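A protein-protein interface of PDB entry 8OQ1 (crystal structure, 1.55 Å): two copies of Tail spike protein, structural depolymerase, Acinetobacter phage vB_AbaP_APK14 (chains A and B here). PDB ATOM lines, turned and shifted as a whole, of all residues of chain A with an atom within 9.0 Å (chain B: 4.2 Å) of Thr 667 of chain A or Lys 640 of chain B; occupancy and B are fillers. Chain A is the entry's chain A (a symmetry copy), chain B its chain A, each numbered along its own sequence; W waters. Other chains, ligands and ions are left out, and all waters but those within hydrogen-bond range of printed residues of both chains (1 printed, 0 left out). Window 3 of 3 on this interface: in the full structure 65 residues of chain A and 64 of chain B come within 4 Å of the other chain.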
ATOM      1  N   GLU A 630       9.419  28.141  13.446  1.00  0.00           N
ATOM      2  CA  GLU A 630       8.162  27.498  13.846  1.00  0.00           C
ATOM      3  C   GLU A 630       7.851  27.810  15.331  1.00  0.00           C
ATOM      4  O   GLU A 630       8.661  27.412  16.190  1.00  0.00           O
ATOM      5  CB  GLU A 630       8.273  25.995  13.663  1.00  0.00           C
ATOM      6  CG  GLU A 630       6.948  25.294  13.879  1.00  0.00           C
ATOM      7  CD  GLU A 630       6.951  23.807  13.567  1.00  0.00           C
ATOM      8  OE1 GLU A 630       7.662  23.370  12.623  1.00  0.00           O
ATOM      9  OE2 GLU A 630       6.287  23.078  14.331  1.00  0.00           O
ATOM     10  N   ARG A 632       4.881  27.613  18.461  1.00  0.00           N
ATOM     11  CA  ARG A 632       3.655  26.911  18.906  1.00  0.00           C
ATOM     12  C   ARG A 632       3.259  27.468  20.274  1.00  0.00           C
ATOM     13  O   ARG A 632       4.190  27.684  21.079  1.00  0.00           O
ATOM     14  CB  ARG A 632       4.008  25.433  18.946  1.00  0.00           C
ATOM     15  CG  ARG A 632       4.491  24.951  17.579  1.00  0.00           C
ATOM     16  CD  ARG A 632       4.720  23.485  17.622  1.00  0.00           C
ATOM     17  NE  ARG A 632       5.847  23.137  18.489  1.00  0.00           N
ATOM     18  CZ  ARG A 632       7.099  22.934  18.101  1.00  0.00           C
ATOM     19  NH1 ARG A 632       7.469  23.070  16.837  1.00  0.00           N
ATOM     20  NH2 ARG A 632       7.993  22.543  18.980  1.00  0.00           N
ATOM     21  N   SER A 636      -2.778  25.566  21.947  1.00  0.00           N
ATOM     22  CA  SER A 636      -3.145  25.855  20.538  1.00  0.00           C
ATOM     23  C   SER A 636      -2.954  24.601  19.686  1.00  0.00           C
ATOM     24  O   SER A 636      -2.053  23.807  20.019  1.00  0.00           O
ATOM     25  CB  SER A 636      -2.315  26.926  19.994  1.00  0.00           C
ATOM     26  OG  SER A 636      -2.759  27.179  18.675  1.00  0.00           O
ATOM     27  N   VAL A 637      -3.688  24.487  18.574  1.00  0.00           N
ATOM     28  CA  VAL A 637      -3.360  23.463  17.518  1.00  0.00           C
ATOM     29  C   VAL A 637      -2.627  24.146  16.337  1.00  0.00           C
ATOM     30  O   VAL A 637      -2.430  23.467  15.320  1.00  0.00           O
ATOM     31  CB  VAL A 637      -4.573  22.640  17.012  1.00  0.00           C
ATOM     32  CG1 VAL A 637      -5.152  21.723  18.081  1.00  0.00           C
ATOM     33  CG2 VAL A 637      -5.643  23.512  16.376  1.00  0.00           C
ATOM     34  N   ALA A 639       0.695  26.053  14.488  1.00  0.00           N
ATOM     35  CA  ALA A 639       2.164  26.272  14.532  1.00  0.00           C
ATOM     36  C   ALA A 639       2.448  27.327  13.451  1.00  0.00           C
ATOM     37  O   ALA A 639       2.201  27.025  12.253  1.00  0.00           O
ATOM     38  CB  ALA A 639       2.917  24.966  14.331  1.00  0.00           C
ATOM     39  N   MET A 664       9.839  16.757  11.404  1.00  0.00           N
ATOM     40  CA  MET A 664       9.026  17.702  12.203  1.00  0.00           C
ATOM     41  C   MET A 664       7.917  16.909  12.926  1.00  0.00           C
ATOM     42  O   MET A 664       7.995  15.675  12.909  1.00  0.00           O
ATOM     43  CB  MET A 664       8.517  18.825  11.277  1.00  0.00           C
ATOM     44  CG  MET A 664       9.679  19.488  10.491  1.00  0.00           C
ATOM     45  SD  MET A 664       9.347  21.090   9.734  1.00  0.00           S
ATOM     46  CE  MET A 664       7.995  20.687   8.618  1.00  0.00           C
ATOM     47  N   LEU A 665       6.917  17.570  13.504  1.00  0.00           N
ATOM     48  CA  LEU A 665       5.963  16.902  14.427  1.00  0.00           C
ATOM     49  C   LEU A 665       5.072  15.928  13.652  1.00  0.00           C
ATOM     50  O   LEU A 665       4.455  16.340  12.601  1.00  0.00           O
ATOM     51  CB  LEU A 665       5.134  17.956  15.181  1.00  0.00           C
ATOM     52  CG  LEU A 665       5.922  18.954  16.049  1.00  0.00           C
ATOM     53  CD1 LEU A 665       4.972  19.862  16.802  1.00  0.00           C
ATOM     54  CD2 LEU A 665       6.826  18.251  17.049  1.00  0.00           C
ATOM     55  N   GLY A 666       4.953  14.705  14.171  1.00  0.00           N
ATOM     56  CA  GLY A 666       4.096  13.641  13.622  1.00  0.00           C
ATOM     57  C   GLY A 666       2.623  14.020  13.571  1.00  0.00           C
ATOM     58  O   GLY A 666       1.942  13.571  12.632  1.00  0.00           O
ATOM     59  N   THR A 667       2.131  14.773  14.559  1.00  0.00           N
ATOM     60  CA  THR A 667       0.694  15.150  14.718  1.00  0.00           C
ATOM     61  C   THR A 667       0.381  16.388  13.905  1.00  0.00           C
ATOM     62  O   THR A 667      -0.811  16.774  13.891  1.00  0.00           O
ATOM     63  CB  THR A 667       0.351  15.418  16.199  1.00  0.00           C
ATOM     64  OG1 THR A 667       1.067  16.575  16.636  1.00  0.00           O
ATOM     65  CG2 THR A 667       0.745  14.249  17.076  1.00  0.00           C
ATOM     66  N   VAL A 668       1.343  16.946  13.150  1.00  0.00           N
ATOM     67  CA  VAL A 668       1.082  18.226  12.450  1.00  0.00           C
ATOM     68  C   VAL A 668       0.967  18.009  10.929  1.00  0.00           C
ATOM     69  O   VAL A 668       1.858  17.347  10.394  1.00  0.00           O
ATOM     70  CB  VAL A 668       2.115  19.307  12.832  1.00  0.00           C
ATOM     71  CG1 VAL A 668       1.892  20.596  12.039  1.00  0.00           C
ATOM     72  CG2 VAL A 668       2.084  19.618  14.332  1.00  0.00           C
ATOM     73  N   SER A 669      -0.051  18.646  10.315  1.00  0.00           N
ATOM     74  CA  SER A 669      -0.214  18.868   8.833  1.00  0.00           C
ATOM     75  C   SER A 669       0.524  20.147   8.454  1.00  0.00           C
ATOM     76  O   SER A 669       0.059  21.214   8.837  1.00  0.00           O
ATOM     77  CB  SER A 669      -1.703  19.025   8.458  1.00  0.00           C
ATOM     78  OG  SER A 669      -2.335  17.756   8.506  1.00  0.00           O
ATOM     79  N   TYR A 670       1.694  20.038   7.841  1.00  0.00           N
ATOM     80  CA  TYR A 670       2.600  21.183   7.543  1.00  0.00           C
ATOM     81  C   TYR A 670       2.201  21.754   6.181  1.00  0.00           C
ATOM     82  O   TYR A 670       1.759  20.985   5.345  1.00  0.00           O
ATOM     83  CB  TYR A 670       4.061  20.766   7.645  1.00  0.00           C
ATOM     84  CG  TYR A 670       4.519  20.699   9.079  1.00  0.00           C
ATOM     85  CD1 TYR A 670       4.938  21.853   9.693  1.00  0.00           C
ATOM     86  CD2 TYR A 670       4.628  19.500   9.783  1.00  0.00           C
ATOM     87  CE1 TYR A 670       5.360  21.864  11.016  1.00  0.00           C
ATOM     88  CE2 TYR A 670       5.112  19.486  11.090  1.00  0.00           C
ATOM     89  CZ  TYR A 670       5.470  20.681  11.711  1.00  0.00           C
ATOM     90  OH  TYR A 670       5.938  20.738  13.016  1.00  0.00           O
ATOM     91  N   ALA A 688       0.709  25.661  10.249  1.00  0.00           N
ATOM     92  CA  ALA A 688       0.527  24.202  10.322  1.00  0.00           C
ATOM     93  C   ALA A 688      -0.543  23.887  11.389  1.00  0.00           C
ATOM     94  O   ALA A 688      -0.707  24.700  12.355  1.00  0.00           O
ATOM     95  CB  ALA A 688       1.831  23.553  10.666  1.00  0.00           C
ATOM     96  N   ILE A 689      -1.252  22.776  11.231  1.00  0.00           N
ATOM     97  CA  ILE A 689      -2.379  22.422  12.151  1.00  0.00           C
ATOM     98  C   ILE A 689      -2.057  21.087  12.813  1.00  0.00           C
ATOM     99  O   ILE A 689      -1.852  20.077  12.093  1.00  0.00           O
ATOM    100  CB  ILE A 689      -3.725  22.397  11.403  1.00  0.00           C
ATOM    101  CG1 ILE A 689      -4.010  23.727  10.705  1.00  0.00           C
ATOM    102  CG2 ILE A 689      -4.853  22.037  12.378  1.00  0.00           C
ATOM    103  CD1 ILE A 689      -5.141  23.621   9.676  1.00  0.00           C
ATOM    104  N   ALA A 690      -2.178  21.039  14.143  1.00  0.00           N
ATOM    105  CA  ALA A 690      -2.013  19.825  14.969  1.00  0.00           C
ATOM    106  C   ALA A 690      -3.349  19.084  15.113  1.00  0.00           C
ATOM    107  O   ALA A 690      -4.439  19.723  15.018  1.00  0.00           O
ATOM    108  CB  ALA A 690      -1.464  20.164  16.325  1.00  0.00           C
ATOM    109  N   SER A 691      -3.214  17.779  15.309  1.00  0.00           N
ATOM    110  CA  SER A 691      -4.265  16.769  15.623  1.00  0.00           C
ATOM    111  C   SER A 691      -4.737  16.947  17.084  1.00  0.00           C
ATOM    112  O   SER A 691      -5.944  16.725  17.384  1.00  0.00           O
ATOM    113  CB  SER A 691      -3.683  15.386  15.396  1.00  0.00           C
ATOM    114  OG  SER A 691      -4.613  14.549  14.760  1.00  0.00           O
ATOM    115  N   GLN A 692      -3.820  17.361  17.958  1.00  0.00           N
ATOM    116  CA  GLN A 692      -4.041  17.548  19.426  1.00  0.00           C
ATOM    117  C   GLN A 692      -3.376  18.867  19.820  1.00  0.00           C
ATOM    118  O   GLN A 692      -2.326  19.195  19.256  1.00  0.00           O
ATOM    119  CB  GLN A 692      -3.407  16.386  20.202  1.00  0.00           C
ATOM    120  N   PRO A 693      -3.897  19.663  20.793  1.00  0.00           N
ATOM    121  CA  PRO A 693      -3.208  20.904  21.185  1.00  0.00           C
ATOM    122  C   PRO A 693      -1.786  20.670  21.736  1.00  0.00           C
ATOM    123  O   PRO A 693      -1.480  19.578  22.236  1.00  0.00           O
ATOM    124  CB  PRO A 693      -4.139  21.545  22.255  1.00  0.00           C
ATOM    125  CG  PRO A 693      -5.488  20.826  22.081  1.00  0.00           C
ATOM    126  CD  PRO A 693      -5.127  19.438  21.585  1.00  0.00           C
ATOM    127  N   PHE A 694      -0.928  21.700  21.639  1.00  0.00           N
ATOM    128  CA  PHE A 694       0.454  21.684  22.171  1.00  0.00           C
ATOM    129  C   PHE A 694       0.400  21.805  23.700  1.00  0.00           C
ATOM    130  O   PHE A 694      -0.307  22.701  24.232  1.00  0.00           O
ATOM    131  CB  PHE A 694       1.338  22.773  21.562  1.00  0.00           C
ATOM    132  CG  PHE A 694       1.416  22.676  20.060  1.00  0.00           C
ATOM    133  CD1 PHE A 694       1.953  21.547  19.457  1.00  0.00           C
ATOM    134  CD2 PHE A 694       0.879  23.668  19.264  1.00  0.00           C
ATOM    135  CE1 PHE A 694       1.980  21.423  18.068  1.00  0.00           C
ATOM    136  CE2 PHE A 694       0.943  23.559  17.877  1.00  0.00           C
ATOM    137  CZ  PHE A 694       1.494  22.438  17.285  1.00  0.00           C
ATOM    138  N   LEU A 695       1.193  20.963  24.363  1.00  0.00           N
ATOM    139  CA  LEU A 695       1.355  20.963  25.845  1.00  0.00           C
ATOM    140  C   LEU A 695       2.059  22.244  26.345  1.00  0.00           C
ATOM    141  O   LEU A 695       1.745  22.654  27.484  1.00  0.00           O
ATOM    142  CB  LEU A 695       2.094  19.684  26.267  1.00  0.00           C
ATOM    143  CG  LEU A 695       1.311  18.384  26.045  1.00  0.00           C
ATOM    144  CD1 LEU A 695       2.168  17.161  26.378  1.00  0.00           C
ATOM    145  CD2 LEU A 695      -0.010  18.366  26.829  1.00  0.00           C
ATOM    146  N   ASN B 629      -7.875   8.835   3.249  1.00  0.00           N
ATOM    147  CA  ASN B 629      -8.689   8.716   4.495  1.00  0.00           C
ATOM    148  C   ASN B 629      -9.061  10.121   4.945  1.00  0.00           C
ATOM    149  O   ASN B 629      -8.159  10.882   5.175  1.00  0.00           O
ATOM    150  CB  ASN B 629      -7.908   7.997   5.586  1.00  0.00           C
ATOM    151  CG  ASN B 629      -8.790   7.790   6.805  1.00  0.00           C
ATOM    152  OD1 ASN B 629      -8.800   8.641   7.683  1.00  0.00           O
ATOM    153  ND2 ASN B 629      -9.584   6.723   6.774  1.00  0.00           N
ATOM    154  N   GLU B 630     -10.350  10.425   5.088  1.00  0.00           N
ATOM    155  CA  GLU B 630     -10.818  11.658   5.730  1.00  0.00           C
ATOM    156  C   GLU B 630     -11.494  11.332   7.085  1.00  0.00           C
ATOM    157  O   GLU B 630     -12.514  10.616   7.067  1.00  0.00           O
ATOM    158  CB  GLU B 630     -11.817  12.360   4.827  1.00  0.00           C
ATOM    159  CG  GLU B 630     -12.192  13.732   5.350  1.00  0.00           C
ATOM    160  CD  GLU B 630     -13.074  14.552   4.423  1.00  0.00           C
ATOM    161  OE1 GLU B 630     -12.924  14.456   3.175  1.00  0.00           O
ATOM    162  OE2 GLU B 630     -13.964  15.236   4.964  1.00  0.00           O
ATOM    163  N   THR B 631     -10.926  11.820   8.182  1.00  0.00           N
ATOM    164  CA  THR B 631     -11.471  11.614   9.561  1.00  0.00           C
ATOM    165  C   THR B 631     -11.879  12.954  10.161  1.00  0.00           C
ATOM    166  O   THR B 631     -11.044  13.906  10.239  1.00  0.00           O
ATOM    167  CB  THR B 631     -10.445  10.917  10.449  1.00  0.00           C
ATOM    168  OG1 THR B 631     -10.214   9.666   9.812  1.00  0.00           O
ATOM    169  CG2 THR B 631     -10.915  10.683  11.876  1.00  0.00           C
ATOM    170  N   PHE B 638     -11.857  20.477  12.072  1.00  0.00           N
ATOM    171  CA  PHE B 638     -10.701  19.957  11.295  1.00  0.00           C
ATOM    172  C   PHE B 638     -11.065  18.590  10.734  1.00  0.00           C
ATOM    173  O   PHE B 638     -11.568  17.753  11.479  1.00  0.00           O
ATOM    174  CB  PHE B 638      -9.471  19.911  12.210  1.00  0.00           C
ATOM    175  CG  PHE B 638      -9.031  21.250  12.741  1.00  0.00           C
ATOM    176  CD1 PHE B 638      -8.699  22.295  11.880  1.00  0.00           C
ATOM    177  CD2 PHE B 638      -9.005  21.502  14.107  1.00  0.00           C
ATOM    178  CE1 PHE B 638      -8.249  23.515  12.365  1.00  0.00           C
ATOM    179  CE2 PHE B 638      -8.611  22.752  14.576  1.00  0.00           C
ATOM    180  CZ  PHE B 638      -8.224  23.741  13.704  1.00  0.00           C
ATOM    181  N   ALA B 639     -10.733  18.317   9.461  1.00  0.00           N
ATOM    182  CA  ALA B 639     -10.909  16.990   8.815  1.00  0.00           C
ATOM    183  C   ALA B 639      -9.495  16.549   8.407  1.00  0.00           C
ATOM    184  O   ALA B 639      -8.881  17.245   7.556  1.00  0.00           O
ATOM    185  CB  ALA B 639     -11.886  17.073   7.653  1.00  0.00           C
ATOM    186  N   LYS B 640      -8.917  15.608   9.159  1.00  0.00           N
ATOM    187  CA  LYS B 640      -7.566  15.081   8.920  1.00  0.00           C
ATOM    188  C   LYS B 640      -7.620  14.184   7.668  1.00  0.00           C
ATOM    189  O   LYS B 640      -8.481  13.243   7.580  1.00  0.00           O
ATOM    190  CB  LYS B 640      -7.036  14.338  10.147  1.00  0.00           C
ATOM    191  CG  LYS B 640      -5.569  13.960  10.055  1.00  0.00           C
ATOM    192  CD  LYS B 640      -4.556  15.094  10.080  1.00  0.00           C
ATOM    193  CE  LYS B 640      -3.182  14.563  10.499  1.00  0.00           C
ATOM    194  NZ  LYS B 640      -2.097  15.579  10.438  1.00  0.00           N
ATOM    195  N   MET B 641      -6.723  14.454   6.696  1.00  0.00           N
ATOM    196  CA  MET B 641      -6.748  13.781   5.390  1.00  0.00           C
ATOM    197  C   MET B 641      -5.395  13.109   5.206  1.00  0.00           C
ATOM    198  O   MET B 641      -4.379  13.757   5.483  1.00  0.00           O
ATOM    199  CB  MET B 641      -7.117  14.795   4.323  1.00  0.00           C
ATOM    200  CG  MET B 641      -8.586  15.207   4.523  1.00  0.00           C
ATOM    201  SD  MET B 641      -8.973  16.378   3.300  1.00  0.00           S
ATOM    202  CE  MET B 641      -9.686  15.253   2.084  1.00  0.00           C
ATOM    203  N   THR B 685      -0.147  13.925   4.483  1.00  0.00           N
ATOM    204  CA  THR B 685      -1.255  14.349   5.370  1.00  0.00           C
ATOM    205  C   THR B 685      -1.495  15.847   5.162  1.00  0.00           C
ATOM    206  O   THR B 685      -0.513  16.568   4.893  1.00  0.00           O
ATOM    207  CB  THR B 685      -0.906  14.027   6.828  1.00  0.00           C
ATOM    208  OG1 THR B 685      -2.156  14.163   7.503  1.00  0.00           O
ATOM    209  CG2 THR B 685       0.208  14.880   7.424  1.00  0.00           C
ATOM    210  N   ALA B 686      -2.751  16.246   5.227  1.00  0.00           N
ATOM    211  CA  ALA B 686      -3.193  17.645   5.273  1.00  0.00           C
ATOM    212  C   ALA B 686      -4.449  17.688   6.130  1.00  0.00           C
ATOM    213  O   ALA B 686      -5.027  16.622   6.397  1.00  0.00           O
ATOM    214  CB  ALA B 686      -3.397  18.181   3.877  1.00  0.00           C
ATOM    215  N   THR B 687      -4.904  18.890   6.373  1.00  0.00           N
ATOM    216  CA  THR B 687      -6.081  19.166   7.230  1.00  0.00           C
ATOM    217  C   THR B 687      -7.023  20.143   6.516  1.00  0.00           C
ATOM    218  O   THR B 687      -6.583  21.225   6.089  1.00  0.00           O
ATOM    219  CB  THR B 687      -5.578  19.608   8.599  1.00  0.00           C
ATOM    220  OG1 THR B 687      -4.954  18.475   9.191  1.00  0.00           O
ATOM    221  CG2 THR B 687      -6.706  20.062   9.504  1.00  0.00           C
HETATM  222  O   HOH W   1      -0.192  19.314   4.842  1.00  0.00           O
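Hydrophobic or aromatic side chains of chain B that line the printed part of chain A: Phe 638.
Of the 20 printed residues of chain A, 5 touch a printed residue of chain B.
NZ of Lys 640 of chain B sits at hydrogen-bond distance from OG of Ser 669 of chain A, 2.9 Å away.
The side-chain hydroxyl (OG1) of Thr 687 of chain B sits at hydrogen-bond distance from the side-chain hydroxyl (OG) of Ser 669 of chain A (2.8 Å).
Positions printed for both chains: 630 and 639.
Of the 9 pairs that touch across the chains among the printed residues, none has its exchanged pair printed and touching as well.
NZ of Lys 640 of chain B sits close to OG1 of Thr 685 of chain B (3.3 Å).
The backbone carbonyl oxygen (O) of Met 641 of chain B lies within hydrogen-bond range of the side-chain hydroxyl (OG1) of Thr 685 of chain B, at 3.0 Å.
N of Met 641 of chain B is in hydrogen-bond range of O of Ala 686 of chain B, 2.8 Å away.
O of Val 637 of chain A is in hydrogen-bond range of N of Ala 690 of chain A, at 2.7 Å.
O of Thr 667 of chain A lies within hydrogen-bond range of N of Ser 691 of chain A (3.0 Å).
The backbone NH (N) of Ser 669 of chain A lies within hydrogen-bond range of the backbone carbonyl oxygen (O) of Ile 689 of chain A (2.9 Å).
Water W1 bridges the backbone carbonyl oxygen (O) of Tyr 670 of chain A (2.6 Å) and the backbone carbonyl oxygen (O) of Thr 685 of chain B (2.8 Å).
Among the printed residues, pairs that only touch across the chains: Val 637 of chain A with Phe 638 of chain B, Thr 667 of chain A with Lys 640 of chain B, Val 668 of chain A with Lys 640 of chain B, Ser 669 of chain A with Thr 685 of chain B, Ser 669 of chain A with Ala 686 of chain B, Ile 689 of chain A with Phe 638 of chain B and Ile 689 of chain A with Thr 687 of chain B.
Thr 667 of chain A touches just one residue of chain B: Lys 640.
Of chain A, only Thr 667 (3.9 Å), Val 668 (3.9 Å) and Ser 669 (2.9 Å) come within 4 Å of Lys 640 of chain B.
Printed residues of chain B within 4 Å of Val 668 of chain A: Lys 640.
Printed residues of chain A within 4 Å of Thr 685 of chain B: Ser 669.
Printed residues of chain B within 4 Å of Val 637 of chain A: Phe 638.
Printed residues of chain A within 4 Å of Thr 687 of chain B: Ser 669 (2.8 Å) and Ile 689 (3.9 Å).
Met 641 of chain B touches none of the printed residues of chain A.
Leu 665 of chain A touches none of the printed residues of chain B.
The nearest printed residue of chain B that does not touch Thr 667 of chain A is Thr 687 of chain B (6.5 Å).
The nearest printed residue of chain A that does not touch Thr 685 of chain B is Val 668 of chain A (4.2 Å).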
